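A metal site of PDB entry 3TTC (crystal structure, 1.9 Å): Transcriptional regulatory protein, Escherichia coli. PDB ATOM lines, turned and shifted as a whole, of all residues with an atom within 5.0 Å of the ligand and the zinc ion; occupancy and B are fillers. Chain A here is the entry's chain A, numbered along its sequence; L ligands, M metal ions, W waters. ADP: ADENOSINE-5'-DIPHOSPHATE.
OE2 of Glu 526 sits at hydrogen-bond distance from O3' of the ligand. N6 of the ligand lies within hydrogen-bond range of OE1 of Glu 534 (2.6 Å). NH1 of Arg 507 lies within hydrogen-bond range of O2' of the ligand, at 3.4 Å. The backbone NH (N) of Asp 638 sits at hydrogen-bond distance from an oxygen (O1A) of the ligand, at 2.9 Å. N1 of the ligand lies within hydrogen-bond range of ND2 of Asn 612, at 2.9 Å. O1B of the ligand sits at hydrogen-bond distance from N of Gly 414. The backbone NH of Gly 608 lies close to an oxygen (O5') of the ligand, 3.4 Å away. The backbone NH (N) of Ile 415 is in hydrogen-bond range of an oxygen (O1B) of the ligand.
Water W2 lies within hydrogen-bond range of an oxygen (O3A) of the ligand, the side-chain carboxylate (OD2) of Asp 638 and the side-chain amino group (NZ) of Lys 313. Water W3 lies within hydrogen-bond range of the backbone carbonyl oxygen (O) of Gly 506 (2.8 Å), an oxygen (O2') of the ligand (3.0 Å) and the guanidinium group (NH1) of Arg 507 (3.2 Å). Water W1 lies within hydrogen-bond range of the side-chain carboxylate of Glu 534 (2.6 Å), a nitrogen (N6) of the ligand (3.2 Å) and the backbone carbonyl oxygen of His 611 (3.5 Å).
Four residues have an atom within 4 Å of the zinc ion: His 386, His 390, Asp 413 and Asp 638. The nearest printed residue that does not touch the zinc ion is Gly 608 (4.8 Å).
O2B of the ligand is bound to the zinc ion (1.8 Å). The zinc ion is bound by NE2 of His 390. OD1 of Asp 413 binds the zinc ion (2.2 Å). The zinc ion is bound by an oxygen (O2A) of the ligand (2.2 Å). The zinc ion is bound by OD1 of Asp 638, at 2.4 Å. The zinc ion is bound by NE2 of His 386 (2.5 Å).
Gly 506 touches the ligand (CA to O2', 3.7 Å). CE2 of Phe 509 touches C2 of the ligand, at 3.5 Å. Ala 530 touches the ligand (CB to N3, 3.5 Å). Gly 607 touches the ligand (C to O2A, 3.97 Å). CG2 of Val 609 touches N3 of the ligand, 3.4 Å away. CA of Gly 637 touches O1A of the ligand (3.3 Å). Within 4 Å of the ligand: His 386, His 390, Asp 413, Gly 414, Ile 415, Gly 506, Arg 507, Phe 509, Glu 526, Ala 530, Glu 534, Gly 607, Gly 608, Val 609, Asn 612, Gly 637 and Asp 638.
ND1 of His 611 lies close to O of Gly 608 (3.5 Å). OE2 of Glu 526 is in salt-bridge range of NH1 of Arg 507. N of Gly 607 lies within hydrogen-bond range of O of Ala 636 (3.1 Å). O of Asp 413 lies within hydrogen-bond range of N of Gly 506 (2.9 Å). The backbone carbonyl oxygen of Ala 636 sits at hydrogen-bond distance from a ring nitrogen (ND1) of His 390, 3.5 Å away.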
ATOM      1  N   LEU A 312      24.139  -7.585 -14.371  1.00  0.00           N
ATOM      2  CA  LEU A 312      24.312  -8.650 -13.386  1.00  0.00           C
ATOM      3  C   LEU A 312      23.132  -9.586 -13.502  1.00  0.00           C
ATOM      4  O   LEU A 312      22.037  -9.140 -13.873  1.00  0.00           O
ATOM      5  CB  LEU A 312      24.337  -8.067 -11.967  1.00  0.00           C
ATOM      6  CG  LEU A 312      25.561  -7.309 -11.407  1.00  0.00           C
ATOM      7  CD1 LEU A 312      26.794  -8.181 -11.432  1.00  0.00           C
ATOM      8  CD2 LEU A 312      25.823  -6.033 -12.136  1.00  0.00           C
ATOM      9  N   LYS A 313      23.340 -10.879 -13.235  1.00  0.00           N
ATOM     10  CA  LYS A 313      22.269 -11.868 -13.265  1.00  0.00           C
ATOM     11  C   LYS A 313      21.485 -11.745 -14.574  1.00  0.00           C
ATOM     12  O   LYS A 313      20.240 -11.883 -14.606  1.00  0.00           O
ATOM     13  CB  LYS A 313      21.331 -11.674 -12.064  1.00  0.00           C
ATOM     14  CG  LYS A 313      22.033 -11.858 -10.721  1.00  0.00           C
ATOM     15  CD  LYS A 313      21.003 -11.749  -9.640  1.00  0.00           C
ATOM     16  CE  LYS A 313      21.471 -12.335  -8.331  1.00  0.00           C
ATOM     17  NZ  LYS A 313      22.192 -11.327  -7.517  1.00  0.00           N
ATOM     18  N   HIS A 386      16.612   1.728 -14.748  1.00  0.00           N
ATOM     19  CA  HIS A 386      16.709   0.441 -14.028  1.00  0.00           C
ATOM     20  C   HIS A 386      15.479   0.187 -13.157  1.00  0.00           C
ATOM     21  O   HIS A 386      14.835  -0.850 -13.251  1.00  0.00           O
ATOM     22  CB  HIS A 386      17.970   0.500 -13.150  1.00  0.00           C
ATOM     23  CG  HIS A 386      18.437  -0.825 -12.654  1.00  0.00           C
ATOM     24  ND1 HIS A 386      19.181  -1.693 -13.425  1.00  0.00           N
ATOM     25  CD2 HIS A 386      18.325  -1.414 -11.430  1.00  0.00           C
ATOM     26  CE1 HIS A 386      19.475  -2.773 -12.713  1.00  0.00           C
ATOM     27  NE2 HIS A 386      18.967  -2.625 -11.493  1.00  0.00           N
ATOM     28  N   HIS A 390      12.348  -2.624 -13.231  1.00  0.00           N
ATOM     29  CA  HIS A 390      11.908  -3.475 -12.097  1.00  0.00           C
ATOM     30  C   HIS A 390      10.410  -3.364 -11.842  1.00  0.00           C
ATOM     31  O   HIS A 390       9.717  -4.370 -11.731  1.00  0.00           O
ATOM     32  CB  HIS A 390      12.587  -3.083 -10.774  1.00  0.00           C
ATOM     33  CG  HIS A 390      13.970  -3.635 -10.624  1.00  0.00           C
ATOM     34  ND1 HIS A 390      14.289  -4.942 -10.921  1.00  0.00           N
ATOM     35  CD2 HIS A 390      15.107  -3.081 -10.116  1.00  0.00           C
ATOM     36  CE1 HIS A 390      15.572  -5.161 -10.665  1.00  0.00           C
ATOM     37  NE2 HIS A 390      16.077  -4.042 -10.172  1.00  0.00           N
ATOM     38  N   ASP A 413      16.944  -2.126  -4.001  1.00  0.00           N
ATOM     39  CA  ASP A 413      18.048  -2.985  -4.488  1.00  0.00           C
ATOM     40  C   ASP A 413      19.394  -2.479  -4.064  1.00  0.00           C
ATOM     41  O   ASP A 413      19.494  -1.765  -3.043  1.00  0.00           O
ATOM     42  CB  ASP A 413      17.972  -3.302  -6.030  1.00  0.00           C
ATOM     43  CG  ASP A 413      18.033  -2.064  -6.915  1.00  0.00           C
ATOM     44  OD1 ASP A 413      17.901  -2.238  -8.171  1.00  0.00           O
ATOM     45  OD2 ASP A 413      18.188  -0.926  -6.401  1.00  0.00           O
ATOM     46  N   GLY A 414      20.424  -2.865  -4.813  1.00  0.00           N
ATOM     47  CA  GLY A 414      21.798  -2.416  -4.517  1.00  0.00           C
ATOM     48  C   GLY A 414      22.003  -1.049  -5.135  1.00  0.00           C
ATOM     49  O   GLY A 414      21.983  -0.047  -4.426  1.00  0.00           O
ATOM     50  N   ILE A 415      22.218  -1.008  -6.447  1.00  0.00           N
ATOM     51  CA  ILE A 415      22.469   0.238  -7.169  1.00  0.00           C
ATOM     52  C   ILE A 415      21.918   0.092  -8.575  1.00  0.00           C
ATOM     53  O   ILE A 415      22.147  -0.931  -9.245  1.00  0.00           O
ATOM     54  CB  ILE A 415      23.991   0.562  -7.357  1.00  0.00           C
ATOM     55  CG1 ILE A 415      24.742   0.690  -6.042  1.00  0.00           C
ATOM     56  CG2 ILE A 415      24.215   1.869  -8.183  1.00  0.00           C
ATOM     57  CD1 ILE A 415      24.235   1.809  -5.142  1.00  0.00           C
ATOM     58  N   GLY A 416      21.231   1.127  -9.023  1.00  0.00           N
ATOM     59  CA  GLY A 416      20.900   1.286 -10.426  1.00  0.00           C
ATOM     60  C   GLY A 416      20.918   2.774 -10.711  1.00  0.00           C
ATOM     61  O   GLY A 416      20.642   3.594  -9.821  1.00  0.00           O
ATOM     62  N   GLY A 506      20.247  -1.790  -0.276  1.00  0.00           N
ATOM     63  CA  GLY A 506      21.202  -2.882  -0.034  1.00  0.00           C
ATOM     64  C   GLY A 506      22.364  -2.448   0.843  1.00  0.00           C
ATOM     65  O   GLY A 506      22.818  -3.210   1.731  1.00  0.00           O
ATOM     66  N   ARG A 507      22.834  -1.212   0.624  1.00  0.00           N
ATOM     67  CA  ARG A 507      23.959  -0.719   1.427  1.00  0.00           C
ATOM     68  C   ARG A 507      23.516  -0.383   2.858  1.00  0.00           C
ATOM     69  O   ARG A 507      24.321  -0.477   3.788  1.00  0.00           O
ATOM     70  CB  ARG A 507      24.659   0.485   0.774  1.00  0.00           C
ATOM     71  CG  ARG A 507      25.303   0.187  -0.591  1.00  0.00           C
ATOM     72  CD  ARG A 507      26.502  -0.817  -0.499  1.00  0.00           C
ATOM     73  NE  ARG A 507      26.007  -2.197  -0.427  1.00  0.00           N
ATOM     74  CZ  ARG A 507      25.547  -2.897  -1.469  1.00  0.00           C
ATOM     75  NH1 ARG A 507      25.077  -4.130  -1.280  1.00  0.00           N
ATOM     76  NH2 ARG A 507      25.527  -2.374  -2.701  1.00  0.00           N
ATOM     77  N   PHE A 509      21.155  -2.142   4.498  1.00  0.00           N
ATOM     78  CA  PHE A 509      21.270  -3.488   5.101  1.00  0.00           C
ATOM     79  C   PHE A 509      22.680  -3.800   5.539  1.00  0.00           C
ATOM     80  O   PHE A 509      22.872  -4.294   6.634  1.00  0.00           O
ATOM     81  CB  PHE A 509      20.787  -4.598   4.136  1.00  0.00           C
ATOM     82  CG  PHE A 509      19.326  -4.909   4.286  1.00  0.00           C
ATOM     83  CD1 PHE A 509      18.375  -4.024   3.811  1.00  0.00           C
ATOM     84  CD2 PHE A 509      18.917  -6.071   4.925  1.00  0.00           C
ATOM     85  CE1 PHE A 509      16.985  -4.315   3.933  1.00  0.00           C
ATOM     86  CE2 PHE A 509      17.547  -6.356   5.078  1.00  0.00           C
ATOM     87  CZ  PHE A 509      16.586  -5.468   4.583  1.00  0.00           C
ATOM     88  N   GLU A 526      28.222 -11.402  -3.186  1.00  0.00           N
ATOM     89  CA  GLU A 526      27.298 -10.264  -3.212  1.00  0.00           C
ATOM     90  C   GLU A 526      25.975 -10.598  -2.511  1.00  0.00           C
ATOM     91  O   GLU A 526      25.343 -11.615  -2.783  1.00  0.00           O
ATOM     92  CB  GLU A 526      27.077  -9.761  -4.659  1.00  0.00           C
ATOM     93  CG  GLU A 526      25.982  -8.674  -4.812  1.00  0.00           C
ATOM     94  CD  GLU A 526      26.456  -7.261  -4.428  1.00  0.00           C
ATOM     95  OE1 GLU A 526      27.346  -6.712  -5.129  1.00  0.00           O
ATOM     96  OE2 GLU A 526      25.902  -6.674  -3.444  1.00  0.00           O
ATOM     97  N   GLY A 527      25.571  -9.716  -1.595  1.00  0.00           N
ATOM     98  CA  GLY A 527      24.352  -9.921  -0.820  1.00  0.00           C
ATOM     99  C   GLY A 527      24.563 -10.726   0.454  1.00  0.00           C
ATOM    100  O   GLY A 527      23.623 -10.966   1.198  1.00  0.00           O
ATOM    101  N   ALA A 530      23.429  -9.009   3.776  1.00  0.00           N
ATOM    102  CA  ALA A 530      21.984  -8.835   3.796  1.00  0.00           C
ATOM    103  C   ALA A 530      21.271 -10.153   4.106  1.00  0.00           C
ATOM    104  O   ALA A 530      20.328 -10.168   4.903  1.00  0.00           O
ATOM    105  CB  ALA A 530      21.495  -8.264   2.446  1.00  0.00           C
ATOM    106  N   CYS A 531      21.718 -11.238   3.481  1.00  0.00           N
ATOM    107  CA  CYS A 531      21.115 -12.550   3.701  1.00  0.00           C
ATOM    108  C   CYS A 531      21.347 -13.022   5.140  1.00  0.00           C
ATOM    109  O   CYS A 531      20.456 -13.622   5.756  1.00  0.00           O
ATOM    110  CB  CYS A 531      21.685 -13.580   2.710  1.00  0.00           C
ATOM    111  SG  CYS A 531      21.120 -13.242   1.013  1.00  0.00           S
ATOM    112  N   GLU A 534      19.014 -11.003   7.392  1.00  0.00           N
ATOM    113  CA  GLU A 534      17.638 -11.521   7.279  1.00  0.00           C
ATOM    114  C   GLU A 534      17.494 -12.834   8.034  1.00  0.00           C
ATOM    115  O   GLU A 534      16.495 -13.036   8.721  1.00  0.00           O
ATOM    116  CB  GLU A 534      17.224 -11.746   5.824  1.00  0.00           C
ATOM    117  CG  GLU A 534      15.740 -12.169   5.701  1.00  0.00           C
ATOM    118  CD  GLU A 534      15.367 -12.674   4.308  1.00  0.00           C
ATOM    119  OE1 GLU A 534      16.147 -12.428   3.363  1.00  0.00           O
ATOM    120  OE2 GLU A 534      14.267 -13.289   4.166  1.00  0.00           O
ATOM    121  N   GLY A 607      12.787  -5.041  -7.259  1.00  0.00           N
ATOM    122  CA  GLY A 607      14.201  -4.887  -6.853  1.00  0.00           C
ATOM    123  C   GLY A 607      14.641  -6.103  -6.043  1.00  0.00           C
ATOM    124  O   GLY A 607      13.818  -6.767  -5.415  1.00  0.00           O
ATOM    125  N   GLY A 608      15.932  -6.404  -6.058  1.00  0.00           N
ATOM    126  CA  GLY A 608      16.391  -7.662  -5.434  1.00  0.00           C
ATOM    127  C   GLY A 608      16.195  -7.715  -3.922  1.00  0.00           C
ATOM    128  O   GLY A 608      16.119  -8.819  -3.355  1.00  0.00           O
ATOM    129  N   VAL A 609      16.130  -6.566  -3.258  1.00  0.00           N
ATOM    130  CA  VAL A 609      15.898  -6.531  -1.808  1.00  0.00           C
ATOM    131  C   VAL A 609      14.507  -7.136  -1.467  1.00  0.00           C
ATOM    132  O   VAL A 609      14.287  -7.656  -0.387  1.00  0.00           O
ATOM    133  CB  VAL A 609      16.072  -5.100  -1.213  1.00  0.00           C
ATOM    134  CG1 VAL A 609      15.530  -5.023   0.220  1.00  0.00           C
ATOM    135  CG2 VAL A 609      17.536  -4.670  -1.250  1.00  0.00           C
ATOM    136  N   HIS A 611      13.315  -9.776  -2.507  1.00  0.00           N
ATOM    137  CA  HIS A 611      13.468 -11.209  -2.225  1.00  0.00           C
ATOM    138  C   HIS A 611      13.476 -11.489  -0.716  1.00  0.00           C
ATOM    139  O   HIS A 611      13.348 -12.637  -0.295  1.00  0.00           O
ATOM    140  CB  HIS A 611      14.753 -11.766  -2.860  1.00  0.00           C
ATOM    141  CG  HIS A 611      14.605 -12.130  -4.317  1.00  0.00           C
ATOM    142  ND1 HIS A 611      15.414 -11.618  -5.304  1.00  0.00           N
ATOM    143  CD2 HIS A 611      13.749 -12.983  -4.935  1.00  0.00           C
ATOM    144  CE1 HIS A 611      15.070 -12.139  -6.467  1.00  0.00           C
ATOM    145  NE2 HIS A 611      14.053 -12.961  -6.279  1.00  0.00           N
ATOM    146  N   ASN A 612      13.667 -10.445   0.099  1.00  0.00           N
ATOM    147  CA  ASN A 612      13.659 -10.599   1.561  1.00  0.00           C
ATOM    148  C   ASN A 612      12.237 -10.898   2.054  1.00  0.00           C
ATOM    149  O   ASN A 612      11.354 -10.052   2.018  1.00  0.00           O
ATOM    150  CB  ASN A 612      14.238  -9.316   2.192  1.00  0.00           C
ATOM    151  CG  ASN A 612      14.441  -9.422   3.701  1.00  0.00           C
ATOM    152  OD1 ASN A 612      13.526  -9.823   4.438  1.00  0.00           O
ATOM    153  ND2 ASN A 612      15.634  -9.025   4.162  1.00  0.00           N
ATOM    154  N   ALA A 636      12.480 -10.983  -8.532  1.00  0.00           N
ATOM    155  CA  ALA A 636      12.334  -9.590  -8.155  1.00  0.00           C
ATOM    156  C   ALA A 636      13.601  -8.793  -8.556  1.00  0.00           C
ATOM    157  O   ALA A 636      13.530  -7.577  -8.800  1.00  0.00           O
ATOM    158  CB  ALA A 636      12.114  -9.463  -6.624  1.00  0.00           C
ATOM    159  N   GLY A 637      14.719  -9.498  -8.594  1.00  0.00           N
ATOM    160  CA  GLY A 637      16.009  -8.893  -8.894  1.00  0.00           C
ATOM    161  C   GLY A 637      16.268  -8.733 -10.394  1.00  0.00           C
ATOM    162  O   GLY A 637      15.359  -8.766 -11.238  1.00  0.00           O
ATOM    163  N   ASP A 638      17.535  -8.567 -10.722  1.00  0.00           N
ATOM    164  CA  ASP A 638      17.931  -8.186 -12.067  1.00  0.00           C
ATOM    165  C   ASP A 638      17.580  -9.219 -13.133  1.00  0.00           C
ATOM    166  O   ASP A 638      17.554  -8.889 -14.335  1.00  0.00           O
ATOM    167  CB  ASP A 638      19.423  -7.836 -12.112  1.00  0.00           C
ATOM    168  CG  ASP A 638      19.744  -6.493 -11.485  1.00  0.00           C
ATOM    169  OD1 ASP A 638      18.818  -5.706 -11.136  1.00  0.00           O
ATOM    170  OD2 ASP A 638      20.962  -6.236 -11.330  1.00  0.00           O
HETATM  171  PB  ADP L   1      21.043  -4.448  -8.577  1.00  0.00           P
HETATM  172  O1B ADP L   1      21.458  -3.888  -7.238  1.00  0.00           O
HETATM  173  O2B ADP L   1      19.999  -3.667  -9.275  1.00  0.00           O
HETATM  174  O3B ADP L   1      22.248  -4.684  -9.460  1.00  0.00           O
HETATM  175  PA  ADP L   1      19.142  -6.596  -7.860  1.00  0.00           P
HETATM  176  O1A ADP L   1      19.135  -8.086  -8.329  1.00  0.00           O
HETATM  177  O2A ADP L   1      17.991  -5.667  -8.120  1.00  0.00           O
HETATM  178  O3A ADP L   1      20.543  -5.974  -8.359  1.00  0.00           O
HETATM  179  O5' ADP L   1      19.347  -6.612  -6.251  1.00  0.00           O
HETATM  180  C5' ADP L   1      20.381  -7.418  -5.697  1.00  0.00           C
HETATM  181  C4' ADP L   1      20.778  -6.775  -4.380  1.00  0.00           C
HETATM  182  O4' ADP L   1      19.692  -6.899  -3.454  1.00  0.00           O
HETATM  183  C3' ADP L   1      21.924  -7.508  -3.686  1.00  0.00           C
HETATM  184  O3' ADP L   1      23.189  -7.082  -4.197  1.00  0.00           O
HETATM  185  C2' ADP L   1      21.735  -7.049  -2.261  1.00  0.00           C
HETATM  186  O2' ADP L   1      22.189  -5.685  -2.265  1.00  0.00           O
HETATM  187  C1' ADP L   1      20.224  -7.037  -2.118  1.00  0.00           C
HETATM  188  N9  ADP L   1      19.674  -8.250  -1.424  1.00  0.00           N
HETATM  189  C8  ADP L   1      19.704  -9.534  -1.851  1.00  0.00           C
HETATM  190  N7  ADP L   1      19.095 -10.375  -0.948  1.00  0.00           N
HETATM  191  C5  ADP L   1      18.667  -9.584   0.078  1.00  0.00           C
HETATM  192  C6  ADP L   1      17.947  -9.798   1.359  1.00  0.00           C
HETATM  193  N6  ADP L   1      17.566 -11.051   1.717  1.00  0.00           N
HETATM  194  N1  ADP L   1      17.679  -8.714   2.135  1.00  0.00           N
HETATM  195  C2  ADP L   1      18.060  -7.470   1.766  1.00  0.00           C
HETATM  196  N3  ADP L   1      18.722  -7.199   0.622  1.00  0.00           N
HETATM  197  C4  ADP L   1      19.042  -8.204  -0.247  1.00  0.00           C
HETATM  198 ZN    ZN M   1      18.209  -3.962  -9.568  1.00  0.00          ZN
HETATM  199  O   HOH W   1      16.186 -13.903   1.226  1.00  0.00           O
HETATM  200  O   HOH W   2      21.845  -8.208  -9.030  1.00  0.00           O
HETATM  201  O   HOH W   3      23.079  -5.770   0.647  1.00  0.00           O
